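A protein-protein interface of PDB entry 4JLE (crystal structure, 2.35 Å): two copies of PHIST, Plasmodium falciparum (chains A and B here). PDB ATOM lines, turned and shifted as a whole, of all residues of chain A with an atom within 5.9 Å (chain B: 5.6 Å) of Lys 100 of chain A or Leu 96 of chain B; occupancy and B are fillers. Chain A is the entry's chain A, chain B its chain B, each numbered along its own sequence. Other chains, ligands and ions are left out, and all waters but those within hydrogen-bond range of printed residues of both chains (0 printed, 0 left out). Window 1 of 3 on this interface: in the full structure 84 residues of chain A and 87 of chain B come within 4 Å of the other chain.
Hydrophobic or aromatic side chains of chain A within 4 Å of the printed part of chain B: Leu 96, Leu 103 and Trp 131. Of the 13 printed residues of chain B, 7 touch a printed residue of chain A. Hydrophobic or aromatic side chains of chain B that line the printed part of chain A: Leu 96 and Leu 103.
Leu 96 of chain A touches Gly 93 of chain B (CD1 to CA, 3.6 Å). CD2 of Leu 96 of chain A touches CD2 of Leu 96 of chain B, 3.5 Å away. Glu 99 of chain A touches Leu 96 of chain B. Lys 100 of chain A touches Leu 96 of chain B. CD1 of Leu 103 of chain A touches CB of Lys 100 of chain B, 3.98 Å away. CB of Leu 103 of chain A touches CD1 of Leu 103 of chain B, 3.9 Å away. Trp 131 of chain A touches Ala 95 of chain B. Trp 131 of chain A touches Gln 98 of chain B. CA of Glu 99 of chain B touches CZ2 of Trp 131 of chain A (3.9 Å).
The side-chain carboxylate (OE2) of Glu 99 of chain B lies close to the side-chain carboxylate (OE2) of Glu 104 of chain A (2.6 Å). NZ of Lys 100 of chain A is in salt-bridge range of OE1 of Glu 99 of chain B.
Leu 96 of chain B touches its own counterpart, Leu 96 of chain A. Glu 99 of chain A touches Leu 96 of chain B, but with the chains exchanged Leu 96 of chain A does not touch Glu 99 of chain B (7.4 Å). Lys 100 of chain A touches Leu 96 of chain B, but with the chains exchanged Leu 96 of chain A does not touch Lys 100 of chain B (8.9 Å). Leu 103 of chain A touches Lys 100 of chain B, but with the chains exchanged Lys 100 of chain A does not touch Leu 103 of chain B (5.0 Å). Positions printed for both chains: 95, 96, 97, 98, 99, 100, 101 and 103. Of the 11 pairs that touch across the chains among the printed residues, 2 have their exchanged pair printed and touching as well.
Leu 96 of chain B touches three residues of chain A. Of the printed residues of chain A, Glu 99 of chain B touches Lys 100, Glu 104 and Trp 131. Of the printed residues of chain A, Gly 93 of chain B touches Leu 96. Of the printed residues of chain B, Leu 96 of chain A touches Gly 93 and Leu 96. Of the printed residues of chain B, Trp 131 of chain A touches Ala 95, Gln 98 and Glu 99. The nearest residue of chain A that does not touch Leu 96 of chain B is Leu 103 of chain A (4.1 Å).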
ATOM      1  N   ALA A  95      -9.610   9.168  23.995  1.00  0.00           N
ATOM      2  CA  ALA A  95      -9.934   7.798  23.557  1.00  0.00           C
ATOM      3  C   ALA A  95     -11.171   7.769  22.651  1.00  0.00           C
ATOM      4  O   ALA A  95     -11.206   6.976  21.701  1.00  0.00           O
ATOM      5  CB  ALA A  95     -10.126   6.880  24.746  1.00  0.00           C
ATOM      6  N   LEU A  96     -12.168   8.646  22.916  1.00  0.00           N
ATOM      7  CA  LEU A  96     -13.389   8.718  22.086  1.00  0.00           C
ATOM      8  C   LEU A  96     -13.045   9.306  20.738  1.00  0.00           C
ATOM      9  O   LEU A  96     -13.491   8.782  19.722  1.00  0.00           O
ATOM     10  CB  LEU A  96     -14.541   9.503  22.766  1.00  0.00           C
ATOM     11  CG  LEU A  96     -15.081   8.858  24.078  1.00  0.00           C
ATOM     12  CD1 LEU A  96     -16.304   9.554  24.609  1.00  0.00           C
ATOM     13  CD2 LEU A  96     -15.266   7.335  23.966  1.00  0.00           C
ATOM     14  N   LYS A  97     -12.190  10.341  20.729  1.00  0.00           N
ATOM     15  CA  LYS A  97     -11.712  10.994  19.506  1.00  0.00           C
ATOM     16  C   LYS A  97     -10.916   9.964  18.650  1.00  0.00           C
ATOM     17  O   LYS A  97     -11.085   9.945  17.441  1.00  0.00           O
ATOM     18  CB  LYS A  97     -10.893  12.252  19.863  1.00  0.00           C
ATOM     19  CG  LYS A  97     -10.057  12.871  18.748  1.00  0.00           C
ATOM     20  CD  LYS A  97      -8.908  13.730  19.300  1.00  0.00           C
ATOM     21  CE  LYS A  97      -7.926  14.195  18.243  1.00  0.00           C
ATOM     22  NZ  LYS A  97      -6.585  14.513  18.826  1.00  0.00           N
ATOM     23  N   GLN A  98     -10.102   9.088  19.274  1.00  0.00           N
ATOM     24  CA  GLN A  98      -9.324   8.042  18.605  1.00  0.00           C
ATOM     25  C   GLN A  98     -10.273   6.992  18.000  1.00  0.00           C
ATOM     26  O   GLN A  98     -10.085   6.597  16.866  1.00  0.00           O
ATOM     27  CB  GLN A  98      -8.325   7.401  19.581  1.00  0.00           C
ATOM     28  CG  GLN A  98      -7.543   6.201  19.042  1.00  0.00           C
ATOM     29  CD  GLN A  98      -6.493   6.566  18.032  1.00  0.00           C
ATOM     30  OE1 GLN A  98      -6.566   6.175  16.894  1.00  0.00           O
ATOM     31  NE2 GLN A  98      -5.475   7.299  18.400  1.00  0.00           N
ATOM     32  N   GLU A  99     -11.294   6.563  18.741  1.00  0.00           N
ATOM     33  CA  GLU A  99     -12.258   5.609  18.229  1.00  0.00           C
ATOM     34  C   GLU A  99     -13.020   6.193  17.033  1.00  0.00           C
ATOM     35  O   GLU A  99     -13.206   5.473  16.054  1.00  0.00           O
ATOM     36  CB  GLU A  99     -13.231   5.178  19.326  1.00  0.00           C
ATOM     37  CG  GLU A  99     -14.052   3.961  18.917  1.00  0.00           C
ATOM     38  CD  GLU A  99     -15.319   3.729  19.710  1.00  0.00           C
ATOM     39  OE1 GLU A  99     -15.376   4.151  20.890  1.00  0.00           O
ATOM     40  OE2 GLU A  99     -16.250   3.101  19.160  1.00  0.00           O
ATOM     41  N   LYS A 100     -13.424   7.491  17.113  1.00  0.00           N
ATOM     42  CA  LYS A 100     -14.127   8.237  16.064  1.00  0.00           C
ATOM     43  C   LYS A 100     -13.288   8.252  14.777  1.00  0.00           C
ATOM     44  O   LYS A 100     -13.816   7.947  13.716  1.00  0.00           O
ATOM     45  CB  LYS A 100     -14.446   9.665  16.527  1.00  0.00           C
ATOM     46  CG  LYS A 100     -15.024  10.577  15.432  1.00  0.00           C
ATOM     47  CD  LYS A 100     -15.293  11.995  15.968  1.00  0.00           C
ATOM     48  CE  LYS A 100     -15.365  13.023  14.863  1.00  0.00           C
ATOM     49  NZ  LYS A 100     -16.453  14.004  15.106  1.00  0.00           N
ATOM     50  N   PHE A 101     -11.985   8.553  14.880  1.00  0.00           N
ATOM     51  CA  PHE A 101     -11.077   8.547  13.722  1.00  0.00           C
ATOM     52  C   PHE A 101     -10.971   7.135  13.115  1.00  0.00           C
ATOM     53  O   PHE A 101     -10.981   7.005  11.900  1.00  0.00           O
ATOM     54  CB  PHE A 101      -9.680   9.059  14.121  1.00  0.00           C
ATOM     55  CG  PHE A 101      -8.563   8.665  13.179  1.00  0.00           C
ATOM     56  CD1 PHE A 101      -8.354   9.358  11.993  1.00  0.00           C
ATOM     57  CD2 PHE A 101      -7.715   7.602  13.484  1.00  0.00           C
ATOM     58  CE1 PHE A 101      -7.318   8.993  11.123  1.00  0.00           C
ATOM     59  CE2 PHE A 101      -6.683   7.233  12.613  1.00  0.00           C
ATOM     60  CZ  PHE A 101      -6.494   7.931  11.437  1.00  0.00           C
ATOM     61  N   LEU A 102     -10.847   6.093  13.962  1.00  0.00           N
ATOM     62  CA  LEU A 102     -10.696   4.711  13.509  1.00  0.00           C
ATOM     63  C   LEU A 102     -12.002   4.160  12.919  1.00  0.00           C
ATOM     64  O   LEU A 102     -11.943   3.303  12.027  1.00  0.00           O
ATOM     65  CB  LEU A 102     -10.160   3.803  14.621  1.00  0.00           C
ATOM     66  CG  LEU A 102      -8.720   4.114  15.084  1.00  0.00           C
ATOM     67  CD1 LEU A 102      -8.386   3.371  16.397  1.00  0.00           C
ATOM     68  CD2 LEU A 102      -7.698   3.842  13.997  1.00  0.00           C
ATOM     69  N   LEU A 103     -13.176   4.673  13.378  1.00  0.00           N
ATOM     70  CA  LEU A 103     -14.458   4.263  12.805  1.00  0.00           C
ATOM     71  C   LEU A 103     -14.597   4.879  11.411  1.00  0.00           C
ATOM     72  O   LEU A 103     -15.049   4.216  10.475  1.00  0.00           O
ATOM     73  CB  LEU A 103     -15.616   4.694  13.705  1.00  0.00           C
ATOM     74  CG  LEU A 103     -15.918   3.845  14.954  1.00  0.00           C
ATOM     75  CD1 LEU A 103     -16.771   4.634  15.909  1.00  0.00           C
ATOM     76  CD2 LEU A 103     -16.653   2.566  14.596  1.00  0.00           C
ATOM     77  N   GLU A 104     -14.159   6.147  11.275  1.00  0.00           N
ATOM     78  CA  GLU A 104     -14.144   6.893  10.024  1.00  0.00           C
ATOM     79  C   GLU A 104     -13.139   6.268   9.088  1.00  0.00           C
ATOM     80  O   GLU A 104     -13.448   6.123   7.912  1.00  0.00           O
ATOM     81  CB  GLU A 104     -13.826   8.373  10.232  1.00  0.00           C
ATOM     82  CG  GLU A 104     -14.975   9.200  10.783  1.00  0.00           C
ATOM     83  CD  GLU A 104     -14.631  10.595  11.287  1.00  0.00           C
ATOM     84  OE1 GLU A 104     -13.565  11.138  10.912  1.00  0.00           O
ATOM     85  OE2 GLU A 104     -15.461  11.162  12.030  1.00  0.00           O
ATOM     86  N   TYR A 105     -11.962   5.867   9.592  1.00  0.00           N
ATOM     87  CA  TYR A 105     -10.932   5.189   8.782  1.00  0.00           C
ATOM     88  C   TYR A 105     -11.512   3.913   8.172  1.00  0.00           C
ATOM     89  O   TYR A 105     -11.379   3.711   6.972  1.00  0.00           O
ATOM     90  CB  TYR A 105      -9.670   4.859   9.609  1.00  0.00           C
ATOM     91  CG  TYR A 105      -8.625   4.102   8.818  1.00  0.00           C
ATOM     92  CD1 TYR A 105      -7.707   4.775   8.012  1.00  0.00           C
ATOM     93  CD2 TYR A 105      -8.597   2.706   8.815  1.00  0.00           C
ATOM     94  CE1 TYR A 105      -6.773   4.080   7.240  1.00  0.00           C
ATOM     95  CE2 TYR A 105      -7.689   2.000   8.020  1.00  0.00           C
ATOM     96  CZ  TYR A 105      -6.757   2.691   7.262  1.00  0.00           C
ATOM     97  OH  TYR A 105      -5.835   1.995   6.516  1.00  0.00           O
ATOM     98  N   TRP A 131     -29.226  14.127  12.642  1.00  0.00           N
ATOM     99  CA  TRP A 131     -28.381  15.091  13.326  1.00  0.00           C
ATOM    100  C   TRP A 131     -29.179  16.282  13.854  1.00  0.00           C
ATOM    101  O   TRP A 131     -28.838  16.811  14.910  1.00  0.00           O
ATOM    102  CB  TRP A 131     -27.234  15.573  12.448  1.00  0.00           C
ATOM    103  CG  TRP A 131     -26.037  14.661  12.479  1.00  0.00           C
ATOM    104  CD1 TRP A 131     -25.481  14.003  11.421  1.00  0.00           C
ATOM    105  CD2 TRP A 131     -25.272  14.265  13.639  1.00  0.00           C
ATOM    106  NE1 TRP A 131     -24.449  13.184  11.853  1.00  0.00           N
ATOM    107  CE2 TRP A 131     -24.304  13.323  13.208  1.00  0.00           C
ATOM    108  CE3 TRP A 131     -25.344  14.577  15.006  1.00  0.00           C
ATOM    109  CZ2 TRP A 131     -23.411  12.703  14.084  1.00  0.00           C
ATOM    110  CZ3 TRP A 131     -24.413  14.000  15.865  1.00  0.00           C
ATOM    111  CH2 TRP A 131     -23.466  13.071  15.405  1.00  0.00           C
ATOM    112  N   ARG B  52     -20.000  19.126  13.398  1.00  0.00           N
ATOM    113  CA  ARG B  52     -19.026  19.423  14.440  1.00  0.00           C
ATOM    114  C   ARG B  52     -19.203  20.880  14.885  1.00  0.00           C
ATOM    115  O   ARG B  52     -19.247  21.145  16.075  1.00  0.00           O
ATOM    116  CB  ARG B  52     -17.619  19.149  13.871  1.00  0.00           C
ATOM    117  CG  ARG B  52     -16.407  19.462  14.732  1.00  0.00           C
ATOM    118  CD  ARG B  52     -15.176  18.941  13.996  1.00  0.00           C
ATOM    119  NE  ARG B  52     -13.901  19.398  14.562  1.00  0.00           N
ATOM    120  CZ  ARG B  52     -12.704  19.006  14.127  1.00  0.00           C
ATOM    121  NH1 ARG B  52     -12.605  18.145  13.120  1.00  0.00           N
ATOM    122  NH2 ARG B  52     -11.599  19.476  14.689  1.00  0.00           N
ATOM    123  N   MET B  91     -21.468  15.022  26.556  1.00  0.00           N
ATOM    124  CA  MET B  91     -22.098  15.403  25.276  1.00  0.00           C
ATOM    125  C   MET B  91     -21.289  14.875  24.083  1.00  0.00           C
ATOM    126  O   MET B  91     -21.893  14.320  23.157  1.00  0.00           O
ATOM    127  CB  MET B  91     -22.317  16.913  25.192  1.00  0.00           C
ATOM    128  CG  MET B  91     -23.362  17.378  26.178  1.00  0.00           C
ATOM    129  SD  MET B  91     -23.848  19.106  26.052  1.00  0.00           S
ATOM    130  CE  MET B  91     -22.540  19.932  26.882  1.00  0.00           C
ATOM    131  N   GLN B  92     -19.925  14.948  24.154  1.00  0.00           N
ATOM    132  CA  GLN B  92     -19.023  14.370  23.143  1.00  0.00           C
ATOM    133  C   GLN B  92     -19.277  12.873  23.033  1.00  0.00           C
ATOM    134  O   GLN B  92     -19.419  12.370  21.926  1.00  0.00           O
ATOM    135  CB  GLN B  92     -17.536  14.627  23.458  1.00  0.00           C
ATOM    136  CG  GLN B  92     -17.090  16.096  23.309  1.00  0.00           C
ATOM    137  CD  GLN B  92     -16.630  16.486  21.911  1.00  0.00           C
ATOM    138  OE1 GLN B  92     -17.388  16.406  20.933  1.00  0.00           O
ATOM    139  NE2 GLN B  92     -15.386  16.973  21.790  1.00  0.00           N
ATOM    140  N   GLY B  93     -19.421  12.209  24.178  1.00  0.00           N
ATOM    141  CA  GLY B  93     -19.703  10.782  24.279  1.00  0.00           C
ATOM    142  C   GLY B  93     -20.972  10.358  23.553  1.00  0.00           C
ATOM    143  O   GLY B  93     -20.987   9.354  22.834  1.00  0.00           O
ATOM    144  N   TYR B  94     -22.043  11.139  23.718  1.00  0.00           N
ATOM    145  CA  TYR B  94     -23.314  10.892  23.051  1.00  0.00           C
ATOM    146  C   TYR B  94     -23.211  11.161  21.550  1.00  0.00           C
ATOM    147  O   TYR B  94     -23.763  10.391  20.772  1.00  0.00           O
ATOM    148  CB  TYR B  94     -24.420  11.740  23.680  1.00  0.00           C
ATOM    149  CG  TYR B  94     -25.049  11.047  24.862  1.00  0.00           C
ATOM    150  CD1 TYR B  94     -25.976  10.017  24.683  1.00  0.00           C
ATOM    151  CD2 TYR B  94     -24.678  11.374  26.166  1.00  0.00           C
ATOM    152  CE1 TYR B  94     -26.542   9.358  25.773  1.00  0.00           C
ATOM    153  CE2 TYR B  94     -25.273  10.753  27.264  1.00  0.00           C
ATOM    154  CZ  TYR B  94     -26.201   9.742  27.064  1.00  0.00           C
ATOM    155  OH  TYR B  94     -26.783   9.116  28.145  1.00  0.00           O
ATOM    156  N   ALA B  95     -22.465  12.204  21.155  1.00  0.00           N
ATOM    157  CA  ALA B  95     -22.247  12.538  19.738  1.00  0.00           C
ATOM    158  C   ALA B  95     -21.470  11.440  19.021  1.00  0.00           C
ATOM    159  O   ALA B  95     -21.802  11.162  17.879  1.00  0.00           O
ATOM    160  CB  ALA B  95     -21.521  13.866  19.604  1.00  0.00           C
ATOM    161  N   LEU B  96     -20.483  10.779  19.701  1.00  0.00           N
ATOM    162  CA  LEU B  96     -19.689   9.687  19.119  1.00  0.00           C
ATOM    163  C   LEU B  96     -20.570   8.500  18.888  1.00  0.00           C
ATOM    164  O   LEU B  96     -20.493   7.900  17.816  1.00  0.00           O
ATOM    165  CB  LEU B  96     -18.460   9.280  19.977  1.00  0.00           C
ATOM    166  CG  LEU B  96     -17.877   7.836  19.726  1.00  0.00           C
ATOM    167  CD1 LEU B  96     -17.075   7.782  18.442  1.00  0.00           C
ATOM    168  CD2 LEU B  96     -16.981   7.355  20.869  1.00  0.00           C
ATOM    169  N   LYS B  97     -21.425   8.182  19.865  1.00  0.00           N
ATOM    170  CA  LYS B  97     -22.346   7.056  19.785  1.00  0.00           C
ATOM    171  C   LYS B  97     -23.325   7.239  18.562  1.00  0.00           C
ATOM    172  O   LYS B  97     -23.598   6.276  17.825  1.00  0.00           O
ATOM    173  CB  LYS B  97     -23.078   6.930  21.153  1.00  0.00           C
ATOM    174  CG  LYS B  97     -24.329   6.051  21.195  1.00  0.00           C
ATOM    175  CD  LYS B  97     -25.190   6.380  22.416  1.00  0.00           C
ATOM    176  CE  LYS B  97     -26.571   5.776  22.336  1.00  0.00           C
ATOM    177  NZ  LYS B  97     -27.452   6.272  23.427  1.00  0.00           N
ATOM    178  N   GLN B  98     -23.811   8.482  18.356  1.00  0.00           N
ATOM    179  CA  GLN B  98     -24.707   8.837  17.265  1.00  0.00           C
ATOM    180  C   GLN B  98     -23.970   8.702  15.914  1.00  0.00           C
ATOM    181  O   GLN B  98     -24.510   8.119  14.976  1.00  0.00           O
ATOM    182  CB  GLN B  98     -25.245  10.272  17.468  1.00  0.00           C
ATOM    183  CG  GLN B  98     -26.115  10.801  16.306  1.00  0.00           C
ATOM    184  CD  GLN B  98     -27.464  10.122  16.166  1.00  0.00           C
ATOM    185  OE1 GLN B  98     -27.758   9.449  15.177  1.00  0.00           O
ATOM    186  NE2 GLN B  98     -28.329  10.319  17.143  1.00  0.00           N
ATOM    187  N   GLU B  99     -22.736   9.225  15.838  1.00  0.00           N
ATOM    188  CA  GLU B  99     -21.934   9.135  14.637  1.00  0.00           C
ATOM    189  C   GLU B  99     -21.622   7.678  14.289  1.00  0.00           C
ATOM    190  O   GLU B  99     -21.706   7.324  13.129  1.00  0.00           O
ATOM    191  CB  GLU B  99     -20.663   9.937  14.768  1.00  0.00           C
ATOM    192  CG  GLU B  99     -20.018  10.177  13.419  1.00  0.00           C
ATOM    193  CD  GLU B  99     -18.572  10.603  13.463  1.00  0.00           C
ATOM    194  OE1 GLU B  99     -18.163  11.230  14.464  1.00  0.00           O
ATOM    195  OE2 GLU B  99     -17.863  10.363  12.464  1.00  0.00           O
ATOM    196  N   LYS B 100     -21.321   6.836  15.292  1.00  0.00           N
ATOM    197  CA  LYS B 100     -21.043   5.407  15.147  1.00  0.00           C
ATOM    198  C   LYS B 100     -22.228   4.696  14.489  1.00  0.00           C
ATOM    199  O   LYS B 100     -22.035   3.965  13.507  1.00  0.00           O
ATOM    200  CB  LYS B 100     -20.703   4.767  16.516  1.00  0.00           C
ATOM    201  CG  LYS B 100     -20.513   3.251  16.460  1.00  0.00           C
ATOM    202  CD  LYS B 100     -20.087   2.662  17.788  1.00  0.00           C
ATOM    203  CE  LYS B 100     -19.992   1.158  17.659  1.00  0.00           C
ATOM    204  NZ  LYS B 100     -20.182   0.461  18.955  1.00  0.00           N
ATOM    205  N   PHE B 101     -23.445   4.940  14.996  1.00  0.00           N
ATOM    206  CA  PHE B 101     -24.652   4.362  14.415  1.00  0.00           C
ATOM    207  C   PHE B 101     -24.854   4.821  12.931  1.00  0.00           C
ATOM    208  O   PHE B 101     -25.215   4.008  12.068  1.00  0.00           O
ATOM    209  CB  PHE B 101     -25.886   4.740  15.259  1.00  0.00           C
ATOM    210  CG  PHE B 101     -27.213   4.612  14.533  1.00  0.00           C
ATOM    211  CD1 PHE B 101     -27.815   3.367  14.352  1.00  0.00           C
ATOM    212  CD2 PHE B 101     -27.861   5.737  14.029  1.00  0.00           C
ATOM    213  CE1 PHE B 101     -29.037   3.252  13.667  1.00  0.00           C
ATOM    214  CE2 PHE B 101     -29.074   5.618  13.341  1.00  0.00           C
ATOM    215  CZ  PHE B 101     -29.649   4.377  13.158  1.00  0.00           C
ATOM    216  N   LEU B 103     -22.527   5.982  10.853  1.00  0.00           N
ATOM    217  CA  LEU B 103     -21.465   5.475   9.988  1.00  0.00           C
ATOM    218  C   LEU B 103     -21.799   4.048   9.588  1.00  0.00           C
ATOM    219  O   LEU B 103     -21.603   3.691   8.438  1.00  0.00           O
ATOM    220  CB  LEU B 103     -20.110   5.510  10.681  1.00  0.00           C
ATOM    221  CG  LEU B 103     -19.366   6.831  10.739  1.00  0.00           C
ATOM    222  CD1 LEU B 103     -18.310   6.779  11.839  1.00  0.00           C
ATOM    223  CD2 LEU B 103     -18.721   7.180   9.396  1.00  0.00           C
